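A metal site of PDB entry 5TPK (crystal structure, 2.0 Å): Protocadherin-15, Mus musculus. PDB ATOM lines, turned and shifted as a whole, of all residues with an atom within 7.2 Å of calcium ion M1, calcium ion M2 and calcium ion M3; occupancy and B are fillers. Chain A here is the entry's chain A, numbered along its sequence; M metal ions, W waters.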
ATOM      1  N   GLU A  21      26.246  14.937  -0.808  1.00  0.00           N
ATOM      2  CA  GLU A  21      25.802  15.435  -2.095  1.00  0.00           C
ATOM      3  C   GLU A  21      24.252  15.389  -2.235  1.00  0.00           C
ATOM      4  O   GLU A  21      23.560  14.696  -1.483  1.00  0.00           O
ATOM      5  CB  GLU A  21      26.422  14.645  -3.247  1.00  0.00           C
ATOM      6  CG  GLU A  21      26.013  13.186  -3.343  1.00  0.00           C
ATOM      7  CD  GLU A  21      26.411  12.532  -4.645  1.00  0.00           C
ATOM      8  OE1 GLU A  21      26.639  11.299  -4.621  1.00  0.00           O
ATOM      9  OE2 GLU A  21      26.469  13.208  -5.695  1.00  0.00           O
ATOM     10  N   GLU A  22      23.764  16.119  -3.243  1.00  0.00           N
ATOM     11  CA  GLU A  22      22.382  16.062  -3.715  1.00  0.00           C
ATOM     12  C   GLU A  22      21.346  16.550  -2.683  1.00  0.00           C
ATOM     13  O   GLU A  22      20.245  16.024  -2.622  1.00  0.00           O
ATOM     14  CB  GLU A  22      22.027  14.670  -4.253  1.00  0.00           C
ATOM     15  CG  GLU A  22      22.989  14.121  -5.328  1.00  0.00           C
ATOM     16  CD  GLU A  22      23.025  14.935  -6.631  1.00  0.00           C
ATOM     17  OE1 GLU A  22      22.275  15.915  -6.807  1.00  0.00           O
ATOM     18  OE2 GLU A  22      23.839  14.578  -7.514  1.00  0.00           O
ATOM     19  N   LEU A  69      24.719  19.777  -4.333  1.00  0.00           N
ATOM     20  CA  LEU A  69      26.082  19.519  -4.840  1.00  0.00           C
ATOM     21  C   LEU A  69      26.086  18.144  -5.500  1.00  0.00           C
ATOM     22  O   LEU A  69      25.382  17.243  -5.076  1.00  0.00           O
ATOM     23  CB  LEU A  69      27.122  19.587  -3.731  1.00  0.00           C
ATOM     24  CG  LEU A  69      27.131  20.900  -2.925  1.00  0.00           C
ATOM     25  CD1 LEU A  69      28.156  20.834  -1.813  1.00  0.00           C
ATOM     26  CD2 LEU A  69      27.398  22.110  -3.820  1.00  0.00           C
ATOM     27  N   ASN A  70      26.890  17.991  -6.549  1.00  0.00           N
ATOM     28  CA  ASN A  70      27.011  16.717  -7.232  1.00  0.00           C
ATOM     29  C   ASN A  70      28.449  16.239  -7.076  1.00  0.00           C
ATOM     30  O   ASN A  70      29.369  16.758  -7.715  1.00  0.00           O
ATOM     31  CB  ASN A  70      26.631  16.872  -8.712  1.00  0.00           C
ATOM     32  CG  ASN A  70      26.679  15.558  -9.474  1.00  0.00           C
ATOM     33  OD1 ASN A  70      26.767  14.475  -8.885  1.00  0.00           O
ATOM     34  ND2 ASN A  70      26.608  15.645 -10.786  1.00  0.00           N
ATOM     35  N   ARG A  71      28.629  15.224  -6.234  1.00  0.00           N
ATOM     36  CA  ARG A  71      29.966  14.655  -6.005  1.00  0.00           C
ATOM     37  C   ARG A  71      30.628  14.184  -7.297  1.00  0.00           C
ATOM     38  O   ARG A  71      31.849  14.296  -7.461  1.00  0.00           O
ATOM     39  CB  ARG A  71      29.929  13.523  -4.998  1.00  0.00           C
ATOM     40  CG  ARG A  71      31.308  13.215  -4.438  1.00  0.00           C
ATOM     41  CD  ARG A  71      31.550  11.741  -4.241  1.00  0.00           C
ATOM     42  NE  ARG A  71      31.227  10.891  -5.412  1.00  0.00           N
ATOM     43  CZ  ARG A  71      32.046  10.507  -6.390  1.00  0.00           C
ATOM     44  NH1 ARG A  71      31.588   9.706  -7.367  1.00  0.00           N
ATOM     45  NH2 ARG A  71      33.313  10.886  -6.411  1.00  0.00           N
ATOM     46  N   GLU A  72      29.827  13.639  -8.206  1.00  0.00           N
ATOM     47  CA  GLU A  72      30.318  13.133  -9.484  1.00  0.00           C
ATOM     48  C   GLU A  72      30.889  14.271 -10.351  1.00  0.00           C
ATOM     49  O   GLU A  72      31.696  14.014 -11.222  1.00  0.00           O
ATOM     50  CB  GLU A  72      29.222  12.354 -10.238  1.00  0.00           C
ATOM     51  CG  GLU A  72      29.024  10.905  -9.784  1.00  0.00           C
ATOM     52  CD  GLU A  72      28.376  10.752  -8.415  1.00  0.00           C
ATOM     53  OE1 GLU A  72      27.304  11.330  -8.160  1.00  0.00           O
ATOM     54  OE2 GLU A  72      28.906   9.984  -7.574  1.00  0.00           O
ATOM     55  N   ALA A  73      30.463  15.520 -10.103  1.00  0.00           N
ATOM     56  CA  ALA A  73      30.982  16.682 -10.828  1.00  0.00           C
ATOM     57  C   ALA A  73      32.141  17.341 -10.086  1.00  0.00           C
ATOM     58  O   ALA A  73      33.130  17.713 -10.710  1.00  0.00           O
ATOM     59  CB  ALA A  73      29.870  17.695 -11.085  1.00  0.00           C
ATOM     60  N   LEU A 102      30.318  14.358   0.240  1.00  0.00           N
ATOM     61  CA  LEU A 102      30.227  12.931   0.473  1.00  0.00           C
ATOM     62  C   LEU A 102      29.330  12.254  -0.554  1.00  0.00           C
ATOM     63  O   LEU A 102      28.351  12.841  -0.984  1.00  0.00           O
ATOM     64  CB  LEU A 102      29.674  12.684   1.876  1.00  0.00           C
ATOM     65  CG  LEU A 102      30.590  13.156   2.999  1.00  0.00           C
ATOM     66  CD1 LEU A 102      29.824  13.155   4.311  1.00  0.00           C
ATOM     67  CD2 LEU A 102      31.830  12.271   3.062  1.00  0.00           C
ATOM     68  N   ASP A 103      29.683  11.026  -0.907  1.00  0.00           N
ATOM     69  CA  ASP A 103      28.992  10.266  -1.954  1.00  0.00           C
ATOM     70  C   ASP A 103      27.743   9.597  -1.434  1.00  0.00           C
ATOM     71  O   ASP A 103      27.756   9.086  -0.313  1.00  0.00           O
ATOM     72  CB  ASP A 103      29.894   9.141  -2.478  1.00  0.00           C
ATOM     73  CG  ASP A 103      29.403   8.547  -3.794  1.00  0.00           C
ATOM     74  OD1 ASP A 103      29.136   9.325  -4.729  1.00  0.00           O
ATOM     75  OD2 ASP A 103      29.331   7.319  -3.902  1.00  0.00           O
ATOM     76  N   ILE A 104      26.692   9.574  -2.252  1.00  0.00           N
ATOM     77  CA  ILE A 104      25.568   8.651  -2.102  1.00  0.00           C
ATOM     78  C   ILE A 104      25.450   7.838  -3.373  1.00  0.00           C
ATOM     79  O   ILE A 104      25.895   8.251  -4.436  1.00  0.00           O
ATOM     80  CB  ILE A 104      24.206   9.358  -1.825  1.00  0.00           C
ATOM     81  CG1 ILE A 104      23.702  10.120  -3.076  1.00  0.00           C
ATOM     82  CG2 ILE A 104      24.350  10.312  -0.648  1.00  0.00           C
ATOM     83  CD1 ILE A 104      22.331  10.753  -2.922  1.00  0.00           C
ATOM     84  N   ASP A 105      24.818   6.668  -3.268  1.00  0.00           N
ATOM     85  CA  ASP A 105      24.473   5.886  -4.441  1.00  0.00           C
ATOM     86  C   ASP A 105      23.272   6.497  -5.151  1.00  0.00           C
ATOM     87  O   ASP A 105      22.139   6.210  -4.822  1.00  0.00           O
ATOM     88  CB  ASP A 105      24.175   4.431  -4.071  1.00  0.00           C
ATOM     89  CG  ASP A 105      23.910   3.558  -5.287  1.00  0.00           C
ATOM     90  OD1 ASP A 105      24.165   4.008  -6.432  1.00  0.00           O
ATOM     91  OD2 ASP A 105      23.447   2.420  -5.101  1.00  0.00           O
ATOM     92  N   ASP A 106      23.548   7.362  -6.121  1.00  0.00           N
ATOM     93  CA  ASP A 106      22.489   8.012  -6.918  1.00  0.00           C
ATOM     94  C   ASP A 106      22.647   7.741  -8.412  1.00  0.00           C
ATOM     95  O   ASP A 106      21.982   8.385  -9.206  1.00  0.00           O
ATOM     96  CB  ASP A 106      22.415   9.520  -6.619  1.00  0.00           C
ATOM     97  CG  ASP A 106      23.716  10.267  -6.924  1.00  0.00           C
ATOM     98  OD1 ASP A 106      24.816   9.665  -6.903  1.00  0.00           O
ATOM     99  OD2 ASP A 106      23.649  11.491  -7.179  1.00  0.00           O
ATOM    100  N   ASN A 107      23.511   6.789  -8.782  1.00  0.00           N
ATOM    101  CA  ASN A 107      23.628   6.356 -10.171  1.00  0.00           C
ATOM    102  C   ASN A 107      23.574   4.831 -10.270  1.00  0.00           C
ATOM    103  O   ASN A 107      24.319   4.132  -9.583  1.00  0.00           O
ATOM    104  CB  ASN A 107      24.925   6.829 -10.800  1.00  0.00           C
ATOM    105  CG  ASN A 107      25.056   8.322 -10.801  1.00  0.00           C
ATOM    106  OD1 ASN A 107      24.682   8.991 -11.776  1.00  0.00           O
ATOM    107  ND2 ASN A 107      25.585   8.873  -9.711  1.00  0.00           N
ATOM    108  N   SER A 108      22.691   4.345 -11.108  1.00  0.00           N
ATOM    109  CA  SER A 108      22.695   2.939 -11.507  1.00  0.00           C
ATOM    110  C   SER A 108      23.829   2.683 -12.479  1.00  0.00           C
ATOM    111  O   SER A 108      24.211   3.597 -13.216  1.00  0.00           O
ATOM    112  CB  SER A 108      21.388   2.574 -12.196  1.00  0.00           C
ATOM    113  OG  SER A 108      20.333   2.659 -11.286  1.00  0.00           O
ATOM    114  N   PRO A 109      24.364   1.454 -12.495  1.00  0.00           N
ATOM    115  CA  PRO A 109      25.288   1.122 -13.568  1.00  0.00           C
ATOM    116  C   PRO A 109      24.660   1.409 -14.934  1.00  0.00           C
ATOM    117  O   PRO A 109      23.470   1.221 -15.081  1.00  0.00           O
ATOM    118  CB  PRO A 109      25.557  -0.386 -13.366  1.00  0.00           C
ATOM    119  CG  PRO A 109      25.297  -0.616 -11.933  1.00  0.00           C
ATOM    120  CD  PRO A 109      24.218   0.337 -11.536  1.00  0.00           C
ATOM    121  N   LYS A 136      29.161   0.658 -16.373  1.00  0.00           N
ATOM    122  CA  LYS A 136      29.986   1.481 -15.472  1.00  0.00           C
ATOM    123  C   LYS A 136      29.090   2.161 -14.453  1.00  0.00           C
ATOM    124  O   LYS A 136      28.005   2.632 -14.792  1.00  0.00           O
ATOM    125  CB  LYS A 136      30.761   2.501 -16.280  1.00  0.00           C
ATOM    126  CG  LYS A 136      31.894   1.871 -17.076  1.00  0.00           C
ATOM    127  CD  LYS A 136      32.436   2.817 -18.158  1.00  0.00           C
ATOM    128  CE  LYS A 136      32.952   2.037 -19.365  1.00  0.00           C
ATOM    129  NZ  LYS A 136      33.231   2.962 -20.499  1.00  0.00           N
ATOM    130  N   ASP A 137      29.533   2.170 -13.203  1.00  0.00           N
ATOM    131  CA  ASP A 137      28.861   2.882 -12.141  1.00  0.00           C
ATOM    132  C   ASP A 137      29.732   4.038 -11.670  1.00  0.00           C
ATOM    133  O   ASP A 137      30.793   3.830 -11.096  1.00  0.00           O
ATOM    134  CB  ASP A 137      28.589   1.913 -10.994  1.00  0.00           C
ATOM    135  CG  ASP A 137      27.604   2.455  -9.990  1.00  0.00           C
ATOM    136  OD1 ASP A 137      27.703   3.659  -9.606  1.00  0.00           O
ATOM    137  OD2 ASP A 137      26.712   1.693  -9.554  1.00  0.00           O
ATOM    138  N   VAL A 138      29.252   5.262 -11.889  1.00  0.00           N
ATOM    139  CA  VAL A 138      30.014   6.483 -11.558  1.00  0.00           C
ATOM    140  C   VAL A 138      30.155   6.796 -10.053  1.00  0.00           C
ATOM    141  O   VAL A 138      30.942   7.661  -9.670  1.00  0.00           O
ATOM    142  CB  VAL A 138      29.488   7.729 -12.313  1.00  0.00           C
ATOM    143  CG1 VAL A 138      29.578   7.511 -13.828  1.00  0.00           C
ATOM    144  CG2 VAL A 138      28.068   8.094 -11.917  1.00  0.00           C
ATOM    145  N   ASP A 139      29.398   6.109  -9.200  1.00  0.00           N
ATOM    146  CA  ASP A 139      29.477   6.342  -7.744  1.00  0.00           C
ATOM    147  C   ASP A 139      30.754   5.767  -7.166  1.00  0.00           C
ATOM    148  O   ASP A 139      31.408   4.927  -7.766  1.00  0.00           O
ATOM    149  CB  ASP A 139      28.278   5.758  -7.018  1.00  0.00           C
ATOM    150  CG  ASP A 139      26.971   6.416  -7.431  1.00  0.00           C
ATOM    151  OD1 ASP A 139      26.877   7.669  -7.391  1.00  0.00           O
ATOM    152  OD2 ASP A 139      26.038   5.684  -7.813  1.00  0.00           O
ATOM    153  N   LEU A 140      31.083   6.245  -5.971  1.00  0.00           N
ATOM    154  CA  LEU A 140      32.345   5.927  -5.302  1.00  0.00           C
ATOM    155  C   LEU A 140      32.356   4.490  -4.752  1.00  0.00           C
ATOM    156  O   LEU A 140      31.440   4.078  -4.069  1.00  0.00           O
ATOM    157  CB  LEU A 140      32.561   6.937  -4.155  1.00  0.00           C
ATOM    158  CG  LEU A 140      33.963   7.203  -3.631  1.00  0.00           C
ATOM    159  CD1 LEU A 140      34.858   7.712  -4.744  1.00  0.00           C
ATOM    160  CD2 LEU A 140      33.881   8.226  -2.514  1.00  0.00           C
ATOM    161  N   ALA A 142      31.954   1.619  -6.202  1.00  0.00           N
ATOM    162  CA  ALA A 142      30.949   0.718  -6.729  1.00  0.00           C
ATOM    163  C   ALA A 142      31.673  -0.490  -7.338  1.00  0.00           C
ATOM    164  O   ALA A 142      32.763  -0.346  -7.876  1.00  0.00           O
ATOM    165  CB  ALA A 142      30.110   1.428  -7.759  1.00  0.00           C
ATOM    166  N   ASP A 192      25.309  -2.737  -8.575  1.00  0.00           N
ATOM    167  CA  ASP A 192      26.293  -2.504  -7.521  1.00  0.00           C
ATOM    168  C   ASP A 192      25.950  -3.461  -6.390  1.00  0.00           C
ATOM    169  O   ASP A 192      24.874  -3.389  -5.793  1.00  0.00           O
ATOM    170  CB  ASP A 192      26.303  -1.045  -7.021  1.00  0.00           C
ATOM    171  CG  ASP A 192      27.502  -0.725  -6.106  1.00  0.00           C
ATOM    172  OD1 ASP A 192      28.272  -1.644  -5.739  1.00  0.00           O
ATOM    173  OD2 ASP A 192      27.669   0.470  -5.742  1.00  0.00           O
ATOM    174  N   GLY A 195      25.262  -1.458  -3.436  1.00  0.00           N
ATOM    175  CA  GLY A 195      24.487  -0.253  -3.715  1.00  0.00           C
ATOM    176  C   GLY A 195      23.002  -0.456  -3.476  1.00  0.00           C
ATOM    177  O   GLY A 195      22.557  -1.570  -3.189  1.00  0.00           O
ATOM    178  N   THR A 196      22.248   0.636  -3.588  1.00  0.00           N
ATOM    179  CA  THR A 196      20.810   0.658  -3.383  1.00  0.00           C
ATOM    180  C   THR A 196      19.994   1.100  -4.598  1.00  0.00           C
ATOM    181  O   THR A 196      18.759   0.980  -4.576  1.00  0.00           O
ATOM    182  CB  THR A 196      20.462   1.625  -2.241  1.00  0.00           C
ATOM    183  OG1 THR A 196      20.973   2.935  -2.536  1.00  0.00           O
ATOM    184  CG2 THR A 196      21.043   1.132  -0.919  1.00  0.00           C
ATOM    185  N   MET A 197      20.644   1.638  -5.625  1.00  0.00           N
ATOM    186  CA  MET A 197      19.939   2.063  -6.835  1.00  0.00           C
ATOM    187  C   MET A 197      19.481   0.819  -7.602  1.00  0.00           C
ATOM    188  O   MET A 197      19.985  -0.282  -7.356  1.00  0.00           O
ATOM    189  CB  MET A 197      20.848   2.929  -7.727  1.00  0.00           C
ATOM    190  CG  MET A 197      20.935   4.382  -7.289  1.00  0.00           C
ATOM    191  SD  MET A 197      19.470   5.341  -7.710  1.00  0.00           S
ATOM    192  CE  MET A 197      19.751   5.735  -9.435  1.00  0.00           C
ATOM    193  N   PRO A 198      18.528   0.993  -8.545  1.00  0.00           N
ATOM    194  CA  PRO A 198      18.142  -0.142  -9.390  1.00  0.00           C
ATOM    195  C   PRO A 198      19.309  -0.643 -10.252  1.00  0.00           C
ATOM    196  O   PRO A 198      20.275   0.099 -10.459  1.00  0.00           O
ATOM    197  CB  PRO A 198      17.023   0.427 -10.280  1.00  0.00           C
ATOM    198  CG  PRO A 198      16.563   1.664  -9.595  1.00  0.00           C
ATOM    199  CD  PRO A 198      17.749   2.202  -8.861  1.00  0.00           C
HETATM  200 CA    CA M   1      27.055   9.522  -6.047  1.00  0.00          CA
HETATM  201 CA    CA M   2      25.540  12.821  -7.838  1.00  0.00          CA
HETATM  202 CA    CA M   3      25.724   3.359  -8.029  1.00  0.00          CA
HETATM  203  O   HOH W   1      24.822  12.090  -9.955  1.00  0.00           O
HETATM  204  O   HOH W   2      26.795   2.730  -6.359  1.00  0.00           O
HETATM  205  O   HOH W   3      24.344   1.403  -7.591  1.00  0.00           O
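The backbone NH (N) of Thr 196 is in hydrogen-bond range of the side-chain carboxylate (OD2) of Asp 105. The side-chain carboxylate (OE2) of Glu 72 sits close to the guanidinium group (NH1) of Arg 71 (2.7 Å). The guanidinium group (NE) of Arg 71 sits close to the side-chain carboxylate (OD1) of Asp 103 (2.7 Å). ND2 of Asn 107 lies close to OD1 of Asp 106. OD2 of Asp 105 is in hydrogen-bond range of N of Met 197 (3.0 Å). N of Glu 22 lies within hydrogen-bond range of O of Leu 69 (2.7 Å). The side-chain carboxylate (OD2) of Asp 103 lies within hydrogen-bond range of the backbone NH (N) of Leu 140. N of Glu 21 sits at hydrogen-bond distance from O of Leu 102, at 3.0 Å.
Within 4 Å of calcium ion M1: Glu 21, Glu 72, Asp 103, Ile 104, Asp 106 and Asp 139. Along chain A the residues within 4 Å of calcium ion M1 span positions 21 to 139.
The nearest printed residue that does not touch calcium ion M2 is Arg 71 (4.2 Å).
Of the 26 residues printed, 4 come within 4 Å of calcium ion M3.
Calcium ion M1 is bound by OD1 of Asp 139, at 2.3 Å. OE1 of Glu 21 binds calcium ion M1, 2.3 Å away. Calcium ion M1 is bound by the backbone carbonyl oxygen (O) of Ile 104 (2.4 Å). OD1 of Asp 106 binds calcium ion M1. Calcium ion M1 is bound by the side-chain carboxylate (OE2) of Glu 72, 2.4 Å away. OD1 of Asp 103 binds calcium ion M1 (2.5 Å). Calcium ion M1 is bound by OE1 of Glu 72 (2.8 Å).
Calcium ion M2 is bound by OD1 of Asn 70 (2.3 Å), OE1 of Glu 72 (2.3 Å), water W1 (2.4 Å), OE2 of Glu 21 (2.4 Å), OD2 of Asp 106 (2.4 Å) and OE2 of Glu 22 (2.5 Å).
Calcium ion M3 is bound by water W2 (2.1 Å), O of Asn 107 (2.2 Å), OD1 of Asp 105 (2.3 Å), OD2 of Asp 139 (2.4 Å), water W3 (2.4 Å), OD2 of Asp 137 (2.5 Å) and OD1 of Asp 137 (2.5 Å). Calcium ion M3 has seven donor atoms within binding distance.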
